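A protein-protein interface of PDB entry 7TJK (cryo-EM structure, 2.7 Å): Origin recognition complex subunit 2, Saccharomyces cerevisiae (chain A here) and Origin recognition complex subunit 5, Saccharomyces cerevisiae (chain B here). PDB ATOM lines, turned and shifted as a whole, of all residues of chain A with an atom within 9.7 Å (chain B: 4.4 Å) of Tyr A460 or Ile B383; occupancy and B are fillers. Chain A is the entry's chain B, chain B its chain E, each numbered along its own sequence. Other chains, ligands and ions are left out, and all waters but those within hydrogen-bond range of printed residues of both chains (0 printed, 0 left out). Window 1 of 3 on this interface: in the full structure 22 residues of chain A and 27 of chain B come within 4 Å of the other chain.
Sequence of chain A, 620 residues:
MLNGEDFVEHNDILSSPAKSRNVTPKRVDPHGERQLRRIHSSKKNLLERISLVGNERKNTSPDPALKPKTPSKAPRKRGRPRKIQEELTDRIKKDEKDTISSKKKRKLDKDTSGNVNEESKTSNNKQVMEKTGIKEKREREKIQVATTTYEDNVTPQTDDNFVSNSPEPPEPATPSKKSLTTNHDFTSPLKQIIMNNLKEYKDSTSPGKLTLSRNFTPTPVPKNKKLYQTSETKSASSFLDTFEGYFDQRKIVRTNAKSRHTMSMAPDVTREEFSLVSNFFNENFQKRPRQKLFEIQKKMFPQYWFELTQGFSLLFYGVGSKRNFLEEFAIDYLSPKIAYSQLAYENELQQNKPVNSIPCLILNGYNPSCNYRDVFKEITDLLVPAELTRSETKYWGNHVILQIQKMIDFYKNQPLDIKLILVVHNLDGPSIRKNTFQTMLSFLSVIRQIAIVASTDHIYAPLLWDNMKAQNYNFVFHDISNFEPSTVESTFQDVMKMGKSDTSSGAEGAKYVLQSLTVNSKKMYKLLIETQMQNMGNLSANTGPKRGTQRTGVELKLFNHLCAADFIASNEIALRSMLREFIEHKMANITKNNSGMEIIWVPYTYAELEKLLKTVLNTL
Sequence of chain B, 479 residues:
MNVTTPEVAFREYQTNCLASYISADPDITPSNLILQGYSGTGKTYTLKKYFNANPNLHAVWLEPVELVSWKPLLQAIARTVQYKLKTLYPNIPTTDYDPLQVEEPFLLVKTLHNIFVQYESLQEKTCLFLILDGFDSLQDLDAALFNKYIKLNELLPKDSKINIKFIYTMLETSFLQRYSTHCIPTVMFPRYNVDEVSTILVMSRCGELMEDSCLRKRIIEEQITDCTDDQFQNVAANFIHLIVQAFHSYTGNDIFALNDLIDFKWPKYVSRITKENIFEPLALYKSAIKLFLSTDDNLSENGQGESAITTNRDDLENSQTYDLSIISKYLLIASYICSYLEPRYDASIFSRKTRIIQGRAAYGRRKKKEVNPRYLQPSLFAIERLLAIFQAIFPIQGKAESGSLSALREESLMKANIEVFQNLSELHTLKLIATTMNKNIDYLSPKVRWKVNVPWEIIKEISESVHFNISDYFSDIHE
Among the printed residues, merely in contact across the chains: Tyr A460 with Leu B444, Tyr A246 with Arg B385, Arg A433 with Leu B444, Tyr A460 with Ile B383, Pro A462 with Phe B421, Leu A463 with Phe B421, Asp A428 with Leu B444, Leu A463 with Leu B424, Leu A463 with Trp B450, Tyr A246 with Glu B384, Leu A464 with Leu B444 and Leu A463 with Ile B383.
A ring nitrogen (ND1) of His A458 sits at hydrogen-bond distance from the backbone NH (N) of Tyr A460.
The guanidinium group (NH2) of Arg A433 lies within hydrogen-bond range of the backbone carbonyl oxygen (O) of Asp A428 (2.7 Å).
OG1 of Thr A456 sits at hydrogen-bond distance from OD2 of Asp A428 (2.4 Å).
The side-chain carboxylate (OD2) of Asp A428 lies within hydrogen-bond range of the backbone NH (N) of His A458 (2.4 Å).
The guanidinium group (NH1) of Arg A250 is in hydrogen-bond range of the side-chain hydroxyl (OH) of Tyr A246.
The side-chain carboxylate of Asp A428 is in hydrogen-bond range of the backbone NH of Asp A457 (2.6 Å).
NE2 of His A458 sits at hydrogen-bond distance from O of Leu B444 (3.4 Å).
OE1 of Glu B384 sits at hydrogen-bond distance from OH of Tyr A460 (2.6 Å).
Hydrophobic or aromatic side chains of chain B within 4 Å of the printed part of chain A: Ile B383, Phe B421, Leu B424, Leu B444 and Trp B450.
Along chain B the printed residues that touch a printed residue of chain A span positions 383 to 450.
Hydrophobic or aromatic side chains of chain A within 4 Å of the printed part of chain B: Tyr A246, His A458, Tyr A460, Pro A462, Leu A463 and Leu A464.
Among the printed residues, no Asp or Glu carboxylate lies within 4 Å of a Lys or Arg side-chain nitrogen of the other chain.
Of chain B, only Ile B383 (3.6 Å), Glu B384 (2.6 Å) and Leu B444 (3.3 Å) come within 4 Å of Tyr A460.
Of the printed residues of chain A, Ile B383 touches Tyr A460 and Leu A463.
No residue of chain A comes within 4 Å of Ala B382.
Glu B384 touches just these residues of chain A: Tyr A246 (3.8 Å) and Tyr A460 (2.6 Å).
Printed residues of chain B within 4 Å of Leu A463: Ile B383, Phe B421, Leu B424 and Trp B450.
Of the printed residues of chain A, Arg B385 touches Tyr A246.
Of the printed residues of chain A, Phe B421 touches Pro A462 and Leu A463.
Of the printed residues of chain A, Leu B424 touches Leu A463.
Printed residues of chain B within 4 Å of His A458: Leu B444.
Ile A459 touches none of the printed residues of chain B.
The nearest printed residue of chain A that does not touch Ile B383 is Tyr A246 (6.4 Å).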
ATOM      1  N   TYR A 246     -10.473  10.272 -12.573  1.00  0.00           N
ATOM      2  CA  TYR A 246     -11.891  10.155 -12.898  1.00  0.00           C
ATOM      3  C   TYR A 246     -12.581  11.511 -12.848  1.00  0.00           C
ATOM      4  O   TYR A 246     -13.352  11.860 -13.750  1.00  0.00           O
ATOM      5  CB  TYR A 246     -12.568   9.180 -11.936  1.00  0.00           C
ATOM      6  CG  TYR A 246     -14.069   9.114 -12.089  1.00  0.00           C
ATOM      7  CD1 TYR A 246     -14.644   8.529 -13.207  1.00  0.00           C
ATOM      8  CD2 TYR A 246     -14.910   9.641 -11.120  1.00  0.00           C
ATOM      9  CE1 TYR A 246     -16.017   8.460 -13.353  1.00  0.00           C
ATOM     10  CE2 TYR A 246     -16.285   9.583 -11.256  1.00  0.00           C
ATOM     11  CZ  TYR A 246     -16.832   8.988 -12.372  1.00  0.00           C
ATOM     12  OH  TYR A 246     -18.197   8.930 -12.512  1.00  0.00           O
ATOM     13  N   PHE A 247     -12.320  12.293 -11.795  1.00  0.00           N
ATOM     14  CA  PHE A 247     -12.913  13.623 -11.719  1.00  0.00           C
ATOM     15  C   PHE A 247     -12.274  14.584 -12.715  1.00  0.00           C
ATOM     16  O   PHE A 247     -12.940  15.509 -13.195  1.00  0.00           O
ATOM     17  CB  PHE A 247     -12.804  14.175 -10.298  1.00  0.00           C
ATOM     18  CG  PHE A 247     -13.554  13.374  -9.277  1.00  0.00           C
ATOM     19  CD1 PHE A 247     -14.787  12.821  -9.583  1.00  0.00           C
ATOM     20  CD2 PHE A 247     -13.032  13.181  -8.008  1.00  0.00           C
ATOM     21  CE1 PHE A 247     -15.482  12.079  -8.643  1.00  0.00           C
ATOM     22  CE2 PHE A 247     -13.722  12.444  -7.063  1.00  0.00           C
ATOM     23  CZ  PHE A 247     -14.948  11.892  -7.382  1.00  0.00           C
ATOM     24  N   ARG A 250     -13.640  14.103 -16.442  1.00  0.00           N
ATOM     25  CA  ARG A 250     -15.045  14.479 -16.612  1.00  0.00           C
ATOM     26  C   ARG A 250     -15.220  15.992 -16.637  1.00  0.00           C
ATOM     27  O   ARG A 250     -15.949  16.561 -15.828  1.00  0.00           O
ATOM     28  CB  ARG A 250     -15.893  13.859 -15.513  1.00  0.00           C
ATOM     29  CG  ARG A 250     -16.040  12.362 -15.620  1.00  0.00           C
ATOM     30  CD  ARG A 250     -16.784  11.814 -14.426  1.00  0.00           C
ATOM     31  NE  ARG A 250     -18.221  11.739 -14.660  1.00  0.00           N
ATOM     32  CZ  ARG A 250     -18.828  10.736 -15.277  1.00  0.00           C
ATOM     33  NH1 ARG A 250     -18.152   9.698 -15.743  1.00  0.00           N
ATOM     34  NH2 ARG A 250     -20.149  10.774 -15.431  1.00  0.00           N
ATOM     35  N   TYR A 317     -10.678 -15.792 -14.499  1.00  0.00           N
ATOM     36  CA  TYR A 317     -10.880 -14.479 -15.086  1.00  0.00           C
ATOM     37  C   TYR A 317      -9.622 -14.087 -15.844  1.00  0.00           C
ATOM     38  O   TYR A 317      -8.639 -14.831 -15.886  1.00  0.00           O
ATOM     39  CB  TYR A 317     -11.257 -13.437 -14.025  1.00  0.00           C
ATOM     40  CG  TYR A 317     -10.197 -13.127 -12.993  1.00  0.00           C
ATOM     41  CD1 TYR A 317     -10.030 -13.934 -11.876  1.00  0.00           C
ATOM     42  CD2 TYR A 317      -9.383 -12.006 -13.121  1.00  0.00           C
ATOM     43  CE1 TYR A 317      -9.070 -13.649 -10.929  1.00  0.00           C
ATOM     44  CE2 TYR A 317      -8.418 -11.713 -12.177  1.00  0.00           C
ATOM     45  CZ  TYR A 317      -8.268 -12.538 -11.084  1.00  0.00           C
ATOM     46  OH  TYR A 317      -7.310 -12.253 -10.141  1.00  0.00           O
ATOM     47  N   ASP A 428     -21.132 -14.443 -16.307  1.00  0.00           N
ATOM     48  CA  ASP A 428     -21.662 -13.090 -16.315  1.00  0.00           C
ATOM     49  C   ASP A 428     -22.349 -12.722 -17.626  1.00  0.00           C
ATOM     50  O   ASP A 428     -22.571 -11.535 -17.878  1.00  0.00           O
ATOM     51  CB  ASP A 428     -20.532 -12.108 -16.037  1.00  0.00           C
ATOM     52  CG  ASP A 428     -19.293 -12.422 -16.837  1.00  0.00           C
ATOM     53  OD1 ASP A 428     -19.308 -13.391 -17.622  1.00  0.00           O
ATOM     54  OD2 ASP A 428     -18.284 -11.715 -16.661  1.00  0.00           O
ATOM     55  N   ARG A 433     -26.743 -14.177 -16.021  1.00  0.00           N
ATOM     56  CA  ARG A 433     -26.332 -13.425 -14.839  1.00  0.00           C
ATOM     57  C   ARG A 433     -27.471 -13.175 -13.863  1.00  0.00           C
ATOM     58  O   ARG A 433     -27.233 -12.555 -12.822  1.00  0.00           O
ATOM     59  CB  ARG A 433     -25.754 -12.069 -15.238  1.00  0.00           C
ATOM     60  CG  ARG A 433     -26.718 -11.226 -16.053  1.00  0.00           C
ATOM     61  CD  ARG A 433     -26.082  -9.943 -16.536  1.00  0.00           C
ATOM     62  NE  ARG A 433     -25.136 -10.175 -17.618  1.00  0.00           N
ATOM     63  CZ  ARG A 433     -24.581  -9.212 -18.340  1.00  0.00           C
ATOM     64  NH1 ARG A 433     -24.894  -7.941 -18.153  1.00  0.00           N
ATOM     65  NH2 ARG A 433     -23.690  -9.534 -19.272  1.00  0.00           N
ATOM     66  N   THR A 456     -15.507 -15.869 -16.300  1.00  0.00           N
ATOM     67  CA  THR A 456     -16.161 -14.568 -16.293  1.00  0.00           C
ATOM     68  C   THR A 456     -15.410 -13.589 -17.186  1.00  0.00           C
ATOM     69  O   THR A 456     -14.206 -13.735 -17.414  1.00  0.00           O
ATOM     70  CB  THR A 456     -16.274 -14.015 -14.862  1.00  0.00           C
ATOM     71  OG1 THR A 456     -16.981 -12.776 -14.881  1.00  0.00           O
ATOM     72  CG2 THR A 456     -14.921 -13.794 -14.252  1.00  0.00           C
ATOM     73  N   ASP A 457     -16.130 -12.598 -17.704  1.00  0.00           N
ATOM     74  CA  ASP A 457     -15.553 -11.605 -18.605  1.00  0.00           C
ATOM     75  C   ASP A 457     -15.828 -10.170 -18.187  1.00  0.00           C
ATOM     76  O   ASP A 457     -15.013  -9.290 -18.469  1.00  0.00           O
ATOM     77  CB  ASP A 457     -16.072 -11.816 -20.031  1.00  0.00           C
ATOM     78  CG  ASP A 457     -15.234 -12.803 -20.814  1.00  0.00           C
ATOM     79  OD1 ASP A 457     -14.032 -12.941 -20.503  1.00  0.00           O
ATOM     80  OD2 ASP A 457     -15.771 -13.438 -21.743  1.00  0.00           O
ATOM     81  N   HIS A 458     -16.959  -9.910 -17.536  1.00  0.00           N
ATOM     82  CA  HIS A 458     -17.297  -8.551 -17.137  1.00  0.00           C
ATOM     83  C   HIS A 458     -16.429  -8.102 -15.970  1.00  0.00           C
ATOM     84  O   HIS A 458     -16.150  -8.864 -15.040  1.00  0.00           O
ATOM     85  CB  HIS A 458     -18.776  -8.458 -16.762  1.00  0.00           C
ATOM     86  CG  HIS A 458     -19.360  -7.094 -16.944  1.00  0.00           C
ATOM     87  ND1 HIS A 458     -19.280  -6.117 -15.976  1.00  0.00           N
ATOM     88  CD2 HIS A 458     -20.022  -6.540 -17.986  1.00  0.00           C
ATOM     89  CE1 HIS A 458     -19.873  -5.021 -16.412  1.00  0.00           C
ATOM     90  NE2 HIS A 458     -20.331  -5.251 -17.628  1.00  0.00           N
ATOM     91  N   ILE A 459     -15.998  -6.841 -16.028  1.00  0.00           N
ATOM     92  CA  ILE A 459     -15.100  -6.304 -15.011  1.00  0.00           C
ATOM     93  C   ILE A 459     -15.837  -5.999 -13.707  1.00  0.00           C
ATOM     94  O   ILE A 459     -15.197  -5.842 -12.659  1.00  0.00           O
ATOM     95  CB  ILE A 459     -14.382  -5.067 -15.587  1.00  0.00           C
ATOM     96  CG1 ILE A 459     -13.079  -4.768 -14.836  1.00  0.00           C
ATOM     97  CG2 ILE A 459     -15.297  -3.853 -15.583  1.00  0.00           C
ATOM     98  CD1 ILE A 459     -12.140  -3.859 -15.583  1.00  0.00           C
ATOM     99  N   TYR A 460     -17.170  -5.948 -13.734  1.00  0.00           N
ATOM    100  CA  TYR A 460     -17.983  -5.686 -12.553  1.00  0.00           C
ATOM    101  C   TYR A 460     -18.617  -6.955 -11.994  1.00  0.00           C
ATOM    102  O   TYR A 460     -19.564  -6.872 -11.212  1.00  0.00           O
ATOM    103  CB  TYR A 460     -19.074  -4.664 -12.876  1.00  0.00           C
ATOM    104  CG  TYR A 460     -18.620  -3.223 -12.927  1.00  0.00           C
ATOM    105  CD1 TYR A 460     -17.326  -2.861 -12.570  1.00  0.00           C
ATOM    106  CD2 TYR A 460     -19.488  -2.224 -13.349  1.00  0.00           C
ATOM    107  CE1 TYR A 460     -16.914  -1.547 -12.622  1.00  0.00           C
ATOM    108  CE2 TYR A 460     -19.084  -0.905 -13.409  1.00  0.00           C
ATOM    109  CZ  TYR A 460     -17.798  -0.572 -13.041  1.00  0.00           C
ATOM    110  OH  TYR A 460     -17.395   0.741 -13.098  1.00  0.00           O
ATOM    111  N   ALA A 461     -18.116  -8.125 -12.393  1.00  0.00           N
ATOM    112  CA  ALA A 461     -18.743  -9.388 -12.006  1.00  0.00           C
ATOM    113  C   ALA A 461     -18.765  -9.721 -10.507  1.00  0.00           C
ATOM    114  O   ALA A 461     -19.727 -10.394 -10.095  1.00  0.00           O
ATOM    115  CB  ALA A 461     -18.088 -10.535 -12.788  1.00  0.00           C
ATOM    116  N   PRO A 462     -17.800  -9.322  -9.656  1.00  0.00           N
ATOM    117  CA  PRO A 462     -17.997  -9.505  -8.204  1.00  0.00           C
ATOM    118  C   PRO A 462     -19.191  -8.767  -7.601  1.00  0.00           C
ATOM    119  O   PRO A 462     -19.599  -9.121  -6.488  1.00  0.00           O
ATOM    120  CB  PRO A 462     -16.681  -8.999  -7.613  1.00  0.00           C
ATOM    121  CG  PRO A 462     -15.701  -9.392  -8.609  1.00  0.00           C
ATOM    122  CD  PRO A 462     -16.355  -9.127  -9.928  1.00  0.00           C
ATOM    123  N   LEU A 463     -19.768  -7.775  -8.288  1.00  0.00           N
ATOM    124  CA  LEU A 463     -21.029  -7.187  -7.845  1.00  0.00           C
ATOM    125  C   LEU A 463     -22.195  -8.171  -7.931  1.00  0.00           C
ATOM    126  O   LEU A 463     -23.215  -7.961  -7.266  1.00  0.00           O
ATOM    127  CB  LEU A 463     -21.330  -5.929  -8.668  1.00  0.00           C
ATOM    128  CG  LEU A 463     -22.462  -4.975  -8.277  1.00  0.00           C
ATOM    129  CD1 LEU A 463     -22.241  -4.438  -6.879  1.00  0.00           C
ATOM    130  CD2 LEU A 463     -22.585  -3.848  -9.285  1.00  0.00           C
ATOM    131  N   LEU A 464     -22.057  -9.252  -8.707  1.00  0.00           N
ATOM    132  CA  LEU A 464     -23.132 -10.229  -8.852  1.00  0.00           C
ATOM    133  C   LEU A 464     -23.424 -11.009  -7.576  1.00  0.00           C
ATOM    134  O   LEU A 464     -24.511 -11.584  -7.465  1.00  0.00           O
ATOM    135  CB  LEU A 464     -22.800 -11.221  -9.969  1.00  0.00           C
ATOM    136  CG  LEU A 464     -22.978 -10.777 -11.419  1.00  0.00           C
ATOM    137  CD1 LEU A 464     -22.621 -11.913 -12.359  1.00  0.00           C
ATOM    138  CD2 LEU A 464     -24.400 -10.302 -11.666  1.00  0.00           C
ATOM    139  N   TRP A 465     -22.504 -11.053  -6.616  1.00  0.00           N
ATOM    140  CA  TRP A 465     -22.625 -11.981  -5.500  1.00  0.00           C
ATOM    141  C   TRP A 465     -22.551 -11.238  -4.172  1.00  0.00           C
ATOM    142  O   TRP A 465     -21.585 -10.512  -3.913  1.00  0.00           O
ATOM    143  CB  TRP A 465     -21.541 -13.056  -5.567  1.00  0.00           C
ATOM    144  CG  TRP A 465     -21.385 -13.601  -6.941  1.00  0.00           C
ATOM    145  CD1 TRP A 465     -22.302 -14.318  -7.640  1.00  0.00           C
ATOM    146  CD2 TRP A 465     -20.211 -13.547  -7.756  1.00  0.00           C
ATOM    147  NE1 TRP A 465     -21.797 -14.666  -8.866  1.00  0.00           N
ATOM    148  CE2 TRP A 465     -20.508 -14.215  -8.958  1.00  0.00           C
ATOM    149  CE3 TRP A 465     -18.942 -12.984  -7.593  1.00  0.00           C
ATOM    150  CZ2 TRP A 465     -19.587 -14.335  -9.992  1.00  0.00           C
ATOM    151  CZ3 TRP A 465     -18.028 -13.106  -8.621  1.00  0.00           C
ATOM    152  CH2 TRP A 465     -18.357 -13.770  -9.806  1.00  0.00           C
ATOM    153  N   ALA B 382     -23.816   6.447 -10.770  1.00  0.00           N
ATOM    154  CA  ALA B 382     -23.182   5.288 -11.383  1.00  0.00           C
ATOM    155  C   ALA B 382     -22.241   4.594 -10.399  1.00  0.00           C
ATOM    156  O   ALA B 382     -21.946   5.101  -9.316  1.00  0.00           O
ATOM    157  CB  ALA B 382     -22.424   5.701 -12.645  1.00  0.00           C
ATOM    158  N   ILE B 383     -21.767   3.411 -10.807  1.00  0.00           N
ATOM    159  CA  ILE B 383     -20.889   2.600  -9.965  1.00  0.00           C
ATOM    160  C   ILE B 383     -19.522   3.260  -9.805  1.00  0.00           C
ATOM    161  O   ILE B 383     -18.969   3.312  -8.697  1.00  0.00           O
ATOM    162  CB  ILE B 383     -20.772   1.175 -10.549  1.00  0.00           C
ATOM    163  CG1 ILE B 383     -22.007   0.350 -10.200  1.00  0.00           C
ATOM    164  CG2 ILE B 383     -19.528   0.444 -10.052  1.00  0.00           C
ATOM    165  CD1 ILE B 383     -22.172   0.086  -8.717  1.00  0.00           C
ATOM    166  N   GLU B 384     -18.966   3.786 -10.900  1.00  0.00           N
ATOM    167  CA  GLU B 384     -17.598   4.296 -10.878  1.00  0.00           C
ATOM    168  C   GLU B 384     -17.475   5.570 -10.052  1.00  0.00           C
ATOM    169  O   GLU B 384     -16.459   5.764  -9.378  1.00  0.00           O
ATOM    170  CB  GLU B 384     -17.104   4.529 -12.308  1.00  0.00           C
ATOM    171  CG  GLU B 384     -15.601   4.761 -12.430  1.00  0.00           C
ATOM    172  CD  GLU B 384     -14.818   3.469 -12.595  1.00  0.00           C
ATOM    173  OE1 GLU B 384     -15.423   2.380 -12.498  1.00  0.00           O
ATOM    174  OE2 GLU B 384     -13.597   3.540 -12.837  1.00  0.00           O
ATOM    175  N   ARG B 385     -18.504   6.426 -10.068  1.00  0.00           N
ATOM    176  CA  ARG B 385     -18.524   7.593  -9.187  1.00  0.00           C
ATOM    177  C   ARG B 385     -18.593   7.179  -7.723  1.00  0.00           C
ATOM    178  O   ARG B 385     -17.931   7.789  -6.869  1.00  0.00           O
ATOM    179  CB  ARG B 385     -19.702   8.500  -9.542  1.00  0.00           C
ATOM    180  CG  ARG B 385     -19.710   9.814  -8.784  1.00  0.00           C
ATOM    181  CD  ARG B 385     -21.047  10.521  -8.880  1.00  0.00           C
ATOM    182  NE  ARG B 385     -21.107  11.658  -7.970  1.00  0.00           N
ATOM    183  CZ  ARG B 385     -22.224  12.276  -7.613  1.00  0.00           C
ATOM    184  NH1 ARG B 385     -23.401  11.906  -8.087  1.00  0.00           N
ATOM    185  NH2 ARG B 385     -22.156  13.291  -6.756  1.00  0.00           N
ATOM    186  N   LEU B 386     -19.383   6.140  -7.422  1.00  0.00           N
ATOM    187  CA  LEU B 386     -19.444   5.582  -6.073  1.00  0.00           C
ATOM    188  C   LEU B 386     -18.091   5.071  -5.605  1.00  0.00           C
ATOM    189  O   LEU B 386     -17.664   5.370  -4.487  1.00  0.00           O
ATOM    190  CB  LEU B 386     -20.474   4.455  -6.016  1.00  0.00           C
ATOM    191  CG  LEU B 386     -20.656   3.828  -4.635  1.00  0.00           C
ATOM    192  CD1 LEU B 386     -21.165   4.843  -3.661  1.00  0.00           C
ATOM    193  CD2 LEU B 386     -21.590   2.632  -4.701  1.00  0.00           C
ATOM    194  N   LEU B 387     -17.388   4.326  -6.459  1.00  0.00           N
ATOM    195  CA  LEU B 387     -16.091   3.788  -6.064  1.00  0.00           C
ATOM    196  C   LEU B 387     -15.027   4.879  -5.968  1.00  0.00           C
ATOM    197  O   LEU B 387     -14.151   4.812  -5.096  1.00  0.00           O
ATOM    198  CB  LEU B 387     -15.671   2.695  -7.044  1.00  0.00           C
ATOM    199  CG  LEU B 387     -16.605   1.489  -7.116  1.00  0.00           C
ATOM    200  CD1 LEU B 387     -16.192   0.579  -8.253  1.00  0.00           C
ATOM    201  CD2 LEU B 387     -16.624   0.737  -5.796  1.00  0.00           C
ATOM    202  N   PHE B 421     -16.998  -5.007  -3.692  1.00  0.00           N
ATOM    203  CA  PHE B 421     -18.171  -5.354  -4.487  1.00  0.00           C
ATOM    204  C   PHE B 421     -19.088  -6.326  -3.755  1.00  0.00           C
ATOM    205  O   PHE B 421     -20.312  -6.256  -3.917  1.00  0.00           O
ATOM    206  CB  PHE B 421     -17.740  -5.939  -5.829  1.00  0.00           C
ATOM    207  CG  PHE B 421     -17.202  -4.922  -6.785  1.00  0.00           C
ATOM    208  CD1 PHE B 421     -18.053  -4.227  -7.629  1.00  0.00           C
ATOM    209  CD2 PHE B 421     -15.845  -4.658  -6.840  1.00  0.00           C
ATOM    210  CE1 PHE B 421     -17.556  -3.286  -8.512  1.00  0.00           C
ATOM    211  CE2 PHE B 421     -15.342  -3.719  -7.721  1.00  0.00           C
ATOM    212  CZ  PHE B 421     -16.199  -3.035  -8.558  1.00  0.00           C
ATOM    213  N   LEU B 424     -20.992  -4.156  -1.401  1.00  0.00           N
ATOM    214  CA  LEU B 424     -21.991  -3.388  -2.138  1.00  0.00           C
ATOM    215  C   LEU B 424     -23.193  -4.250  -2.517  1.00  0.00           C
ATOM    216  O   LEU B 424     -24.344  -3.797  -2.432  1.00  0.00           O
ATOM    217  CB  LEU B 424     -21.350  -2.770  -3.379  1.00  0.00           C
ATOM    218  CG  LEU B 424     -22.183  -1.794  -4.210  1.00  0.00           C
ATOM    219  CD1 LEU B 424     -22.863  -0.757  -3.332  1.00  0.00           C
ATOM    220  CD2 LEU B 424     -21.299  -1.126  -5.243  1.00  0.00           C
ATOM    221  N   LEU B 444     -25.060  -5.792 -13.973  1.00  0.00           N
ATOM    222  CA  LEU B 444     -23.925  -5.464 -14.821  1.00  0.00           C
ATOM    223  C   LEU B 444     -24.279  -4.516 -15.956  1.00  0.00           C
ATOM    224  O   LEU B 444     -23.395  -4.146 -16.735  1.00  0.00           O
ATOM    225  CB  LEU B 444     -23.323  -6.748 -15.393  1.00  0.00           C
ATOM    226  CG  LEU B 444     -22.938  -7.828 -14.383  1.00  0.00           C
ATOM    227  CD1 LEU B 444     -22.205  -8.951 -15.074  1.00  0.00           C
ATOM    228  CD2 LEU B 444     -22.082  -7.246 -13.280  1.00  0.00           C
ATOM    229  N   TRP B 450     -28.140   3.868  -9.455  1.00  0.00           N
ATOM    230  CA  TRP B 450     -28.061   3.502  -8.051  1.00  0.00           C
ATOM    231  C   TRP B 450     -28.481   4.686  -7.193  1.00  0.00           C
ATOM    232  O   TRP B 450     -28.260   5.836  -7.567  1.00  0.00           O
ATOM    233  CB  TRP B 450     -26.628   3.086  -7.729  1.00  0.00           C
ATOM    234  CG  TRP B 450     -26.210   1.881  -8.505  1.00  0.00           C
ATOM    235  CD1 TRP B 450     -25.552   1.875  -9.695  1.00  0.00           C
ATOM    236  CD2 TRP B 450     -26.322   0.511  -8.104  1.00  0.00           C
ATOM    237  NE1 TRP B 450     -25.314   0.590 -10.098  1.00  0.00           N
ATOM    238  CE2 TRP B 450     -25.761  -0.269  -9.131  1.00  0.00           C
ATOM    239  CE3 TRP B 450     -26.856  -0.131  -6.987  1.00  0.00           C
ATOM    240  CZ2 TRP B 450     -25.719  -1.658  -9.076  1.00  0.00           C
ATOM    241  CZ3 TRP B 450     -26.811  -1.510  -6.932  1.00  0.00           C
ATOM    242  CH2 TRP B 450     -26.253  -2.259  -7.972  1.00  0.00           C
